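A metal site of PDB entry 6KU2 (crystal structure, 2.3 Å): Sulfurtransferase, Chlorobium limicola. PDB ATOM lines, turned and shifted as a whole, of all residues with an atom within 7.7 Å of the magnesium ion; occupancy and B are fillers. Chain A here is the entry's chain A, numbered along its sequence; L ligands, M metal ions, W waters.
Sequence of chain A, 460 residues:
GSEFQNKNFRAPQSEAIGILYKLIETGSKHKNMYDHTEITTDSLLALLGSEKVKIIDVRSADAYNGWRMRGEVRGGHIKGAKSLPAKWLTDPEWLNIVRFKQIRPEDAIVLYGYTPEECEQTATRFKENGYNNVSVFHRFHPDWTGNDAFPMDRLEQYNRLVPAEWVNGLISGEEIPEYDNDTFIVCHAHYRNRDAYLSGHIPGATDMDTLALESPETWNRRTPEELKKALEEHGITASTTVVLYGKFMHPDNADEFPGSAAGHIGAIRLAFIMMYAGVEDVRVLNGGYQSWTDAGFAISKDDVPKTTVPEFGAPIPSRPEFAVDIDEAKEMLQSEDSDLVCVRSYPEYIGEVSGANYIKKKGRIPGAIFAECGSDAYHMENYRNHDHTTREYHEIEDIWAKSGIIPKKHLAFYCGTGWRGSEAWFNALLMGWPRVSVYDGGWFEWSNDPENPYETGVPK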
ATOM      1  N   GLU A 214      -3.269   5.228  12.440  1.00  0.00           N
ATOM      2  CA  GLU A 214      -3.583   3.901  12.921  1.00  0.00           C
ATOM      3  C   GLU A 214      -2.397   3.285  13.642  1.00  0.00           C
ATOM      4  O   GLU A 214      -1.233   3.675  13.414  1.00  0.00           O
ATOM      5  CB  GLU A 214      -4.089   3.002  11.788  1.00  0.00           C
ATOM      6  CG  GLU A 214      -3.250   2.932  10.550  1.00  0.00           C
ATOM      7  CD  GLU A 214      -3.807   2.004   9.457  1.00  0.00           C
ATOM      8  OE1 GLU A 214      -5.000   1.650   9.491  1.00  0.00           O
ATOM      9  OE2 GLU A 214      -3.041   1.624   8.538  1.00  0.00           O
ATOM     10  N   SER A 215      -2.709   2.391  14.563  1.00  0.00           N
ATOM     11  CA  SER A 215      -1.746   1.804  15.443  1.00  0.00           C
ATOM     12  C   SER A 215      -1.182   0.536  14.822  1.00  0.00           C
ATOM     13  O   SER A 215      -1.941  -0.363  14.447  1.00  0.00           O
ATOM     14  CB  SER A 215      -2.396   1.432  16.773  1.00  0.00           C
ATOM     15  OG  SER A 215      -1.542   0.543  17.506  1.00  0.00           O
ATOM     16  N   THR A 218      -2.668  -2.820  16.907  1.00  0.00           N
ATOM     17  CA  THR A 218      -4.027  -3.326  16.640  1.00  0.00           C
ATOM     18  C   THR A 218      -4.441  -3.207  15.175  1.00  0.00           C
ATOM     19  O   THR A 218      -5.474  -3.729  14.808  1.00  0.00           O
ATOM     20  CB  THR A 218      -5.060  -2.495  17.425  1.00  0.00           C
ATOM     21  OG1 THR A 218      -4.843  -1.122  17.130  1.00  0.00           O
ATOM     22  CG2 THR A 218      -4.928  -2.740  18.943  1.00  0.00           C
ATOM     23  N   TRP A 219      -3.666  -2.480  14.381  1.00  0.00           N
ATOM     24  CA  TRP A 219      -4.109  -1.977  13.067  1.00  0.00           C
ATOM     25  C   TRP A 219      -5.528  -1.394  13.069  1.00  0.00           C
ATOM     26  O   TRP A 219      -6.281  -1.432  12.082  1.00  0.00           O
ATOM     27  CB  TRP A 219      -3.867  -3.012  11.968  1.00  0.00           C
ATOM     28  CG  TRP A 219      -2.430  -3.410  11.827  1.00  0.00           C
ATOM     29  CD1 TRP A 219      -1.959  -4.644  11.941  1.00  0.00           C
ATOM     30  CD2 TRP A 219      -1.303  -2.587  11.530  1.00  0.00           C
ATOM     31  NE1 TRP A 219      -0.610  -4.679  11.742  1.00  0.00           N
ATOM     32  CE2 TRP A 219      -0.175  -3.417  11.499  1.00  0.00           C
ATOM     33  CE3 TRP A 219      -1.123  -1.218  11.281  1.00  0.00           C
ATOM     34  CZ2 TRP A 219       1.083  -2.954  11.238  1.00  0.00           C
ATOM     35  CZ3 TRP A 219       0.145  -0.758  11.030  1.00  0.00           C
ATOM     36  CH2 TRP A 219       1.226  -1.622  11.011  1.00  0.00           C
ATOM     37  N   ASN A 220      -5.861  -0.761  14.158  1.00  0.00           N
ATOM     38  CA  ASN A 220      -7.109  -0.014  14.263  1.00  0.00           C
ATOM     39  C   ASN A 220      -6.765   1.451  14.398  1.00  0.00           C
ATOM     40  O   ASN A 220      -5.598   1.802  14.688  1.00  0.00           O
ATOM     41  CB  ASN A 220      -7.931  -0.524  15.470  1.00  0.00           C
ATOM     42  CG  ASN A 220      -8.701  -1.819  15.164  1.00  0.00           C
ATOM     43  OD1 ASN A 220      -8.609  -2.405  14.052  1.00  0.00           O
ATOM     44  ND2 ASN A 220      -9.473  -2.270  16.157  1.00  0.00           N
ATOM     45  N   ARG A 221      -7.766   2.302  14.156  1.00  0.00           N
ATOM     46  CA  ARG A 221      -7.627   3.737  14.399  1.00  0.00           C
ATOM     47  C   ARG A 221      -7.040   4.023  15.793  1.00  0.00           C
ATOM     48  O   ARG A 221      -7.274   3.324  16.788  1.00  0.00           O
ATOM     49  CB  ARG A 221      -8.981   4.458  14.278  1.00  0.00           C
ATOM     50  CG  ARG A 221     -10.012   4.031  15.331  1.00  0.00           C
ATOM     51  CD  ARG A 221     -11.467   4.152  14.883  1.00  0.00           C
ATOM     52  NE  ARG A 221     -12.351   3.872  16.016  1.00  0.00           N
ATOM     53  CZ  ARG A 221     -12.712   2.652  16.411  1.00  0.00           C
ATOM     54  NH1 ARG A 221     -12.270   1.553  15.781  1.00  0.00           N
ATOM     55  NH2 ARG A 221     -13.512   2.536  17.463  1.00  0.00           N
ATOM     56  N   ARG A 269      -8.577   4.903   3.311  1.00  0.00           N
ATOM     57  CA  ARG A 269      -8.571   4.477   4.715  1.00  0.00           C
ATOM     58  C   ARG A 269      -8.445   5.662   5.634  1.00  0.00           C
ATOM     59  O   ARG A 269      -9.180   5.755   6.625  1.00  0.00           O
ATOM     60  CB  ARG A 269      -7.451   3.459   4.979  1.00  0.00           C
ATOM     61  CG  ARG A 269      -7.068   3.278   6.450  1.00  0.00           C
ATOM     62  CD  ARG A 269      -8.081   2.432   7.194  1.00  0.00           C
ATOM     63  NE  ARG A 269      -7.599   2.105   8.519  1.00  0.00           N
ATOM     64  CZ  ARG A 269      -8.318   1.508   9.475  1.00  0.00           C
ATOM     65  NH1 ARG A 269      -7.755   1.267  10.631  1.00  0.00           N
ATOM     66  NH2 ARG A 269      -9.588   1.173   9.303  1.00  0.00           N
ATOM     67  N   PHE A 272     -11.620   7.665   5.800  1.00  0.00           N
ATOM     68  CA  PHE A 272     -12.499   7.073   6.793  1.00  0.00           C
ATOM     69  C   PHE A 272     -12.160   7.599   8.188  1.00  0.00           C
ATOM     70  O   PHE A 272     -13.020   8.069   8.936  1.00  0.00           O
ATOM     71  CB  PHE A 272     -12.411   5.525   6.757  1.00  0.00           C
ATOM     72  CG  PHE A 272     -12.935   4.862   8.000  1.00  0.00           C
ATOM     73  CD1 PHE A 272     -14.290   4.858   8.292  1.00  0.00           C
ATOM     74  CD2 PHE A 272     -12.084   4.261   8.892  1.00  0.00           C
ATOM     75  CE1 PHE A 272     -14.770   4.262   9.437  1.00  0.00           C
ATOM     76  CE2 PHE A 272     -12.557   3.640  10.020  1.00  0.00           C
ATOM     77  CZ  PHE A 272     -13.905   3.657  10.303  1.00  0.00           C
ATOM     78  N   VAL A 324     -17.055   0.522  13.892  1.00  0.00           N
ATOM     79  CA  VAL A 324     -17.655  -0.557  14.620  1.00  0.00           C
ATOM     80  C   VAL A 324     -16.516  -1.438  15.147  1.00  0.00           C
ATOM     81  O   VAL A 324     -15.480  -1.679  14.462  1.00  0.00           O
ATOM     82  CB  VAL A 324     -18.618  -1.305  13.700  1.00  0.00           C
ATOM     83  CG1 VAL A 324     -18.898  -2.708  14.178  1.00  0.00           C
ATOM     84  CG2 VAL A 324     -19.899  -0.507  13.549  1.00  0.00           C
ATOM     85  N   ASP A 325     -16.714  -1.902  16.376  1.00  0.00           N
ATOM     86  CA  ASP A 325     -15.739  -2.699  17.077  1.00  0.00           C
ATOM     87  C   ASP A 325     -16.336  -4.047  17.343  1.00  0.00           C
ATOM     88  O   ASP A 325     -17.491  -4.300  16.987  1.00  0.00           O
ATOM     89  CB  ASP A 325     -15.242  -1.942  18.306  1.00  0.00           C
ATOM     90  CG  ASP A 325     -14.335  -0.733  17.916  1.00  0.00           C
ATOM     91  OD1 ASP A 325     -13.408  -0.893  17.102  1.00  0.00           O
ATOM     92  OD2 ASP A 325     -14.556   0.385  18.406  1.00  0.00           O
ATOM     93  N   CYS A 415     -12.191  -6.061   6.203  1.00  0.00           N
ATOM     94  CA  CYS A 415     -11.290  -6.845   5.423  1.00  0.00           C
ATOM     95  C   CYS A 415     -10.310  -7.369   6.456  1.00  0.00           C
ATOM     96  O   CYS A 415     -10.738  -7.762   7.486  1.00  0.00           O
ATOM     97  CB  CYS A 415     -10.608  -5.989   4.400  1.00  0.00           C
ATOM     98  SG  CYS A 415      -9.715  -4.663   5.094  1.00  0.00           S
ATOM     99  N   GLY A 416      -9.041  -7.428   6.130  1.00  0.00           N
ATOM    100  CA  GLY A 416      -8.081  -7.844   7.104  1.00  0.00           C
ATOM    101  C   GLY A 416      -7.791  -6.907   8.257  1.00  0.00           C
ATOM    102  O   GLY A 416      -7.897  -7.318   9.354  1.00  0.00           O
ATOM    103  N   THR A 417      -7.497  -5.641   7.988  1.00  0.00           N
ATOM    104  CA  THR A 417      -7.189  -4.624   8.991  1.00  0.00           C
ATOM    105  C   THR A 417      -8.041  -3.387   8.882  1.00  0.00           C
ATOM    106  O   THR A 417      -8.004  -2.548   9.708  1.00  0.00           O
ATOM    107  CB  THR A 417      -5.728  -4.162   8.963  1.00  0.00           C
ATOM    108  OG1 THR A 417      -5.451  -3.553   7.715  1.00  0.00           O
ATOM    109  CG2 THR A 417      -4.817  -5.295   9.181  1.00  0.00           C
ATOM    110  N   GLY A 418      -8.798  -3.294   7.827  1.00  0.00           N
ATOM    111  CA  GLY A 418      -9.725  -2.156   7.649  1.00  0.00           C
ATOM    112  C   GLY A 418      -9.481  -1.234   6.455  1.00  0.00           C
ATOM    113  O   GLY A 418     -10.252  -0.324   6.258  1.00  0.00           O
ATOM    114  N   TRP A 419      -8.436  -1.490   5.651  1.00  0.00           N
ATOM    115  CA  TRP A 419      -8.122  -0.662   4.443  1.00  0.00           C
ATOM    116  C   TRP A 419      -9.126  -0.881   3.291  1.00  0.00           C
ATOM    117  O   TRP A 419      -9.725   0.063   2.783  1.00  0.00           O
ATOM    118  CB  TRP A 419      -6.688  -0.935   3.952  1.00  0.00           C
ATOM    119  CG  TRP A 419      -5.633  -0.202   4.620  1.00  0.00           C
ATOM    120  CD1 TRP A 419      -5.546   0.132   5.939  1.00  0.00           C
ATOM    121  CD2 TRP A 419      -4.469   0.333   3.995  1.00  0.00           C
ATOM    122  NE1 TRP A 419      -4.391   0.828   6.173  1.00  0.00           N
ATOM    123  CE2 TRP A 419      -3.688   0.948   5.000  1.00  0.00           C
ATOM    124  CE3 TRP A 419      -3.949   0.278   2.675  1.00  0.00           C
ATOM    125  CZ2 TRP A 419      -2.432   1.540   4.731  1.00  0.00           C
ATOM    126  CZ3 TRP A 419      -2.675   0.888   2.405  1.00  0.00           C
ATOM    127  CH2 TRP A 419      -1.962   1.525   3.424  1.00  0.00           C
ATOM    128  N   VAL A 438     -17.348   0.900   9.084  1.00  0.00           N
ATOM    129  CA  VAL A 438     -16.217  -0.031   8.948  1.00  0.00           C
ATOM    130  C   VAL A 438     -16.057  -0.793  10.271  1.00  0.00           C
ATOM    131  O   VAL A 438     -15.827  -0.167  11.309  1.00  0.00           O
ATOM    132  CB  VAL A 438     -14.876   0.697   8.567  1.00  0.00           C
ATOM    133  CG1 VAL A 438     -13.718  -0.313   8.486  1.00  0.00           C
ATOM    134  CG2 VAL A 438     -15.017   1.457   7.254  1.00  0.00           C
ATOM    135  N   TYR A 439     -16.177  -2.119  10.261  1.00  0.00           N
ATOM    136  CA  TYR A 439     -15.692  -2.943  11.405  1.00  0.00           C
ATOM    137  C   TYR A 439     -14.128  -2.993  11.371  1.00  0.00           C
ATOM    138  O   TYR A 439     -13.561  -3.783  10.628  1.00  0.00           O
ATOM    139  CB  TYR A 439     -16.303  -4.376  11.444  1.00  0.00           C
ATOM    140  CG  TYR A 439     -15.502  -5.345  12.291  1.00  0.00           C
ATOM    141  CD1 TYR A 439     -15.083  -4.999  13.565  1.00  0.00           C
ATOM    142  CD2 TYR A 439     -15.140  -6.589  11.826  1.00  0.00           C
ATOM    143  CE1 TYR A 439     -14.305  -5.839  14.341  1.00  0.00           C
ATOM    144  CE2 TYR A 439     -14.392  -7.447  12.615  1.00  0.00           C
ATOM    145  CZ  TYR A 439     -13.998  -7.052  13.861  1.00  0.00           C
ATOM    146  OH  TYR A 439     -13.257  -7.814  14.653  1.00  0.00           O
ATOM    147  N   ASP A 440     -13.480  -2.175  12.185  1.00  0.00           N
ATOM    148  CA  ASP A 440     -12.052  -1.849  12.052  1.00  0.00           C
ATOM    149  C   ASP A 440     -11.099  -3.030  12.250  1.00  0.00           C
ATOM    150  O   ASP A 440     -10.225  -3.281  11.421  1.00  0.00           O
ATOM    151  CB  ASP A 440     -11.731  -0.722  13.045  1.00  0.00           C
ATOM    152  CG  ASP A 440     -10.464  -0.018  12.780  1.00  0.00           C
ATOM    153  OD1 ASP A 440      -9.687  -0.461  11.866  1.00  0.00           O
ATOM    154  OD2 ASP A 440     -10.224   0.964  13.515  1.00  0.00           O
ATOM    155  N   GLY A 441     -11.296  -3.779  13.333  1.00  0.00           N
ATOM    156  CA  GLY A 441     -10.467  -4.922  13.698  1.00  0.00           C
ATOM    157  C   GLY A 441     -10.279  -5.936  12.600  1.00  0.00           C
ATOM    158  O   GLY A 441      -9.180  -6.451  12.384  1.00  0.00           O
ATOM    159  N   GLY A 442     -11.375  -6.232  11.890  1.00  0.00           N
ATOM    160  CA  GLY A 442     -11.347  -7.136  10.766  1.00  0.00           C
ATOM    161  C   GLY A 442     -10.931  -8.500  11.214  1.00  0.00           C
ATOM    162  O   GLY A 442     -11.077  -8.847  12.366  1.00  0.00           O
ATOM    163  N   TRP A 443     -10.467  -9.283  10.255  1.00  0.00           N
ATOM    164  CA  TRP A 443      -9.967 -10.627  10.453  1.00  0.00           C
ATOM    165  C   TRP A 443      -8.731 -10.695  11.355  1.00  0.00           C
ATOM    166  O   TRP A 443      -8.575 -11.655  12.108  1.00  0.00           O
ATOM    167  CB  TRP A 443      -9.720 -11.300   9.092  1.00  0.00           C
ATOM    168  CG  TRP A 443      -9.089 -12.654   9.176  1.00  0.00           C
ATOM    169  CD1 TRP A 443      -7.820 -13.004   8.786  1.00  0.00           C
ATOM    170  CD2 TRP A 443      -9.657 -13.841   9.747  1.00  0.00           C
ATOM    171  NE1 TRP A 443      -7.591 -14.306   9.030  1.00  0.00           N
ATOM    172  CE2 TRP A 443      -8.698 -14.859   9.632  1.00  0.00           C
ATOM    173  CE3 TRP A 443     -10.891 -14.137  10.339  1.00  0.00           C
ATOM    174  CZ2 TRP A 443      -8.928 -16.149  10.055  1.00  0.00           C
ATOM    175  CZ3 TRP A 443     -11.102 -15.435  10.782  1.00  0.00           C
ATOM    176  CH2 TRP A 443     -10.127 -16.411  10.647  1.00  0.00           C
ATOM    177  N   PHE A 444      -7.891  -9.669  11.298  1.00  0.00           N
ATOM    178  CA  PHE A 444      -6.729  -9.615  12.136  1.00  0.00           C
ATOM    179  C   PHE A 444      -7.173  -9.591  13.607  1.00  0.00           C
ATOM    180  O   PHE A 444      -6.700 -10.396  14.388  1.00  0.00           O
ATOM    181  CB  PHE A 444      -5.872  -8.384  11.784  1.00  0.00           C
ATOM    182  CG  PHE A 444      -4.671  -8.185  12.662  1.00  0.00           C
ATOM    183  CD1 PHE A 444      -3.561  -9.007  12.538  1.00  0.00           C
ATOM    184  CD2 PHE A 444      -4.659  -7.198  13.625  1.00  0.00           C
ATOM    185  CE1 PHE A 444      -2.445  -8.854  13.358  1.00  0.00           C
ATOM    186  CE2 PHE A 444      -3.537  -7.005  14.424  1.00  0.00           C
ATOM    187  CZ  PHE A 444      -2.433  -7.856  14.305  1.00  0.00           C
ATOM    188  N   GLU A 445      -8.068  -8.679  13.978  1.00  0.00           N
ATOM    189  CA  GLU A 445      -8.550  -8.663  15.370  1.00  0.00           C
ATOM    190  C   GLU A 445      -9.280  -9.963  15.713  1.00  0.00           C
ATOM    191  O   GLU A 445      -9.002 -10.577  16.754  1.00  0.00           O
ATOM    192  CB  GLU A 445      -9.471  -7.479  15.658  1.00  0.00           C
ATOM    193  CG  GLU A 445      -9.909  -7.421  17.116  1.00  0.00           C
ATOM    194  CD  GLU A 445     -10.802  -6.266  17.459  1.00  0.00           C
ATOM    195  OE1 GLU A 445     -10.611  -5.694  18.543  1.00  0.00           O
ATOM    196  OE2 GLU A 445     -11.712  -5.942  16.678  1.00  0.00           O
HETATM  197  C1  LIG L   1      -2.370  -2.013   8.205  1.00  0.00           C
HETATM  198  C2  LIG L   1      -0.156  -2.932   7.872  1.00  0.00           C
HETATM  199  C3  LIG L   1      -0.811  -0.738   6.847  1.00  0.00           C
HETATM  200  C4  LIG L   1      -1.944  -2.931   6.053  1.00  0.00           C
HETATM  201  C5  LIG L   1      -0.841  -3.583   5.125  1.00  0.00           C
HETATM  202  C6  LIG L   1      -2.864  -2.184   5.100  1.00  0.00           C
HETATM  203  C7  LIG L   1      -3.703  -3.070   4.344  1.00  0.00           C
HETATM  204  C8  LIG L   1      -4.534  -5.082   4.141  1.00  0.00           C
HETATM  205  N1  LIG L   1      -1.328  -2.139   7.188  1.00  0.00           N
HETATM  206  O1  LIG L   1      -0.016  -2.768   4.587  1.00  0.00           O
HETATM  207  O2  LIG L   1      -0.892  -4.838   4.983  1.00  0.00           O
HETATM  208  C9  LIG L   1      -3.797  -3.305   2.948  1.00  0.00           C
HETATM  209  N2  LIG L   1      -4.761  -4.374   2.851  1.00  0.00           N
HETATM  210  S1  LIG L   1      -5.991  -6.199   4.738  1.00  0.00           S
HETATM  211  S2  LIG L   1      -7.669  -4.817   4.697  1.00  0.00           S
HETATM  212  N3  LIG L   1      -4.507  -3.972   4.982  1.00  0.00           N
HETATM  213 MG    MG M   1      -8.330  -2.250  11.865  1.00  0.00          MG
HETATM  214  O   HOH W   1      -7.027  -4.558  12.464  1.00  0.00           O
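NH1 of Arg 269 touches the magnesium ion, 3.8 Å away. Gly 441 touches the magnesium ion.
Water W1 bridges O of Gly 441 (2.9 Å) and O of Thr 218 (2.9 Å).
N of Thr 417 sits close to S2 of the ligand (3.4 Å). A nitrogen (N3) of the ligand is in hydrogen-bond range of the side-chain hydroxyl (OG1) of Thr 417, at 2.9 Å. The backbone NH (N) of Gly 418 sits close to a sulfur (S2) of the ligand. A sulfur (S2) of the ligand lies close to the backbone NH of Gly 416 (3.3 Å). N of Trp 419 sits close to S2 of the ligand (3.5 Å). SG of Cys 415 is covalently linked to S2 of the ligand, 2.1 Å away.
The backbone NH of Thr 417 sits close to the side-chain sulfur of Cys 415 (3.8 Å). The side-chain carboxylate of Asp 440 lies within salt-bridge range of the guanidinium group of Arg 269, at 3.8 Å. The guanidinium group (NH1) of Arg 221 is in salt-bridge range of the side-chain carboxylate (OD2) of Asp 440 (3.1 Å). The backbone NH of Asp 440 lies within hydrogen-bond range of the backbone carbonyl oxygen of Val 324, at 3.1 Å. The side-chain amide oxygen (OD1) of Asn 220 lies close to the backbone NH (N) of Gly 441 (3.1 Å). The side-chain hydroxyl of Thr 218 sits close to the backbone NH of Asn 220. The guanidinium group of Arg 269 sits close to the backbone carbonyl oxygen of Trp 219, 3.4 Å away. The guanidinium group of Arg 269 is in salt-bridge range of the side-chain carboxylate of Glu 214 (2.8 Å).
The magnesium ion is bound by the backbone carbonyl oxygen (O) of Thr 417 (2.2 Å), the backbone carbonyl oxygen (O) of Asp 440 (2.2 Å), the side-chain amide oxygen (OD1) of Asn 220 (2.2 Å), the backbone carbonyl oxygen (O) of Trp 219 (2.2 Å) and the side-chain carboxylate (OD1) of Asp 440 (2.2 Å). The magnesium ion has five donor atoms within binding distance. Slightly farther from the magnesium ion lies water W1 (2.7 Å).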
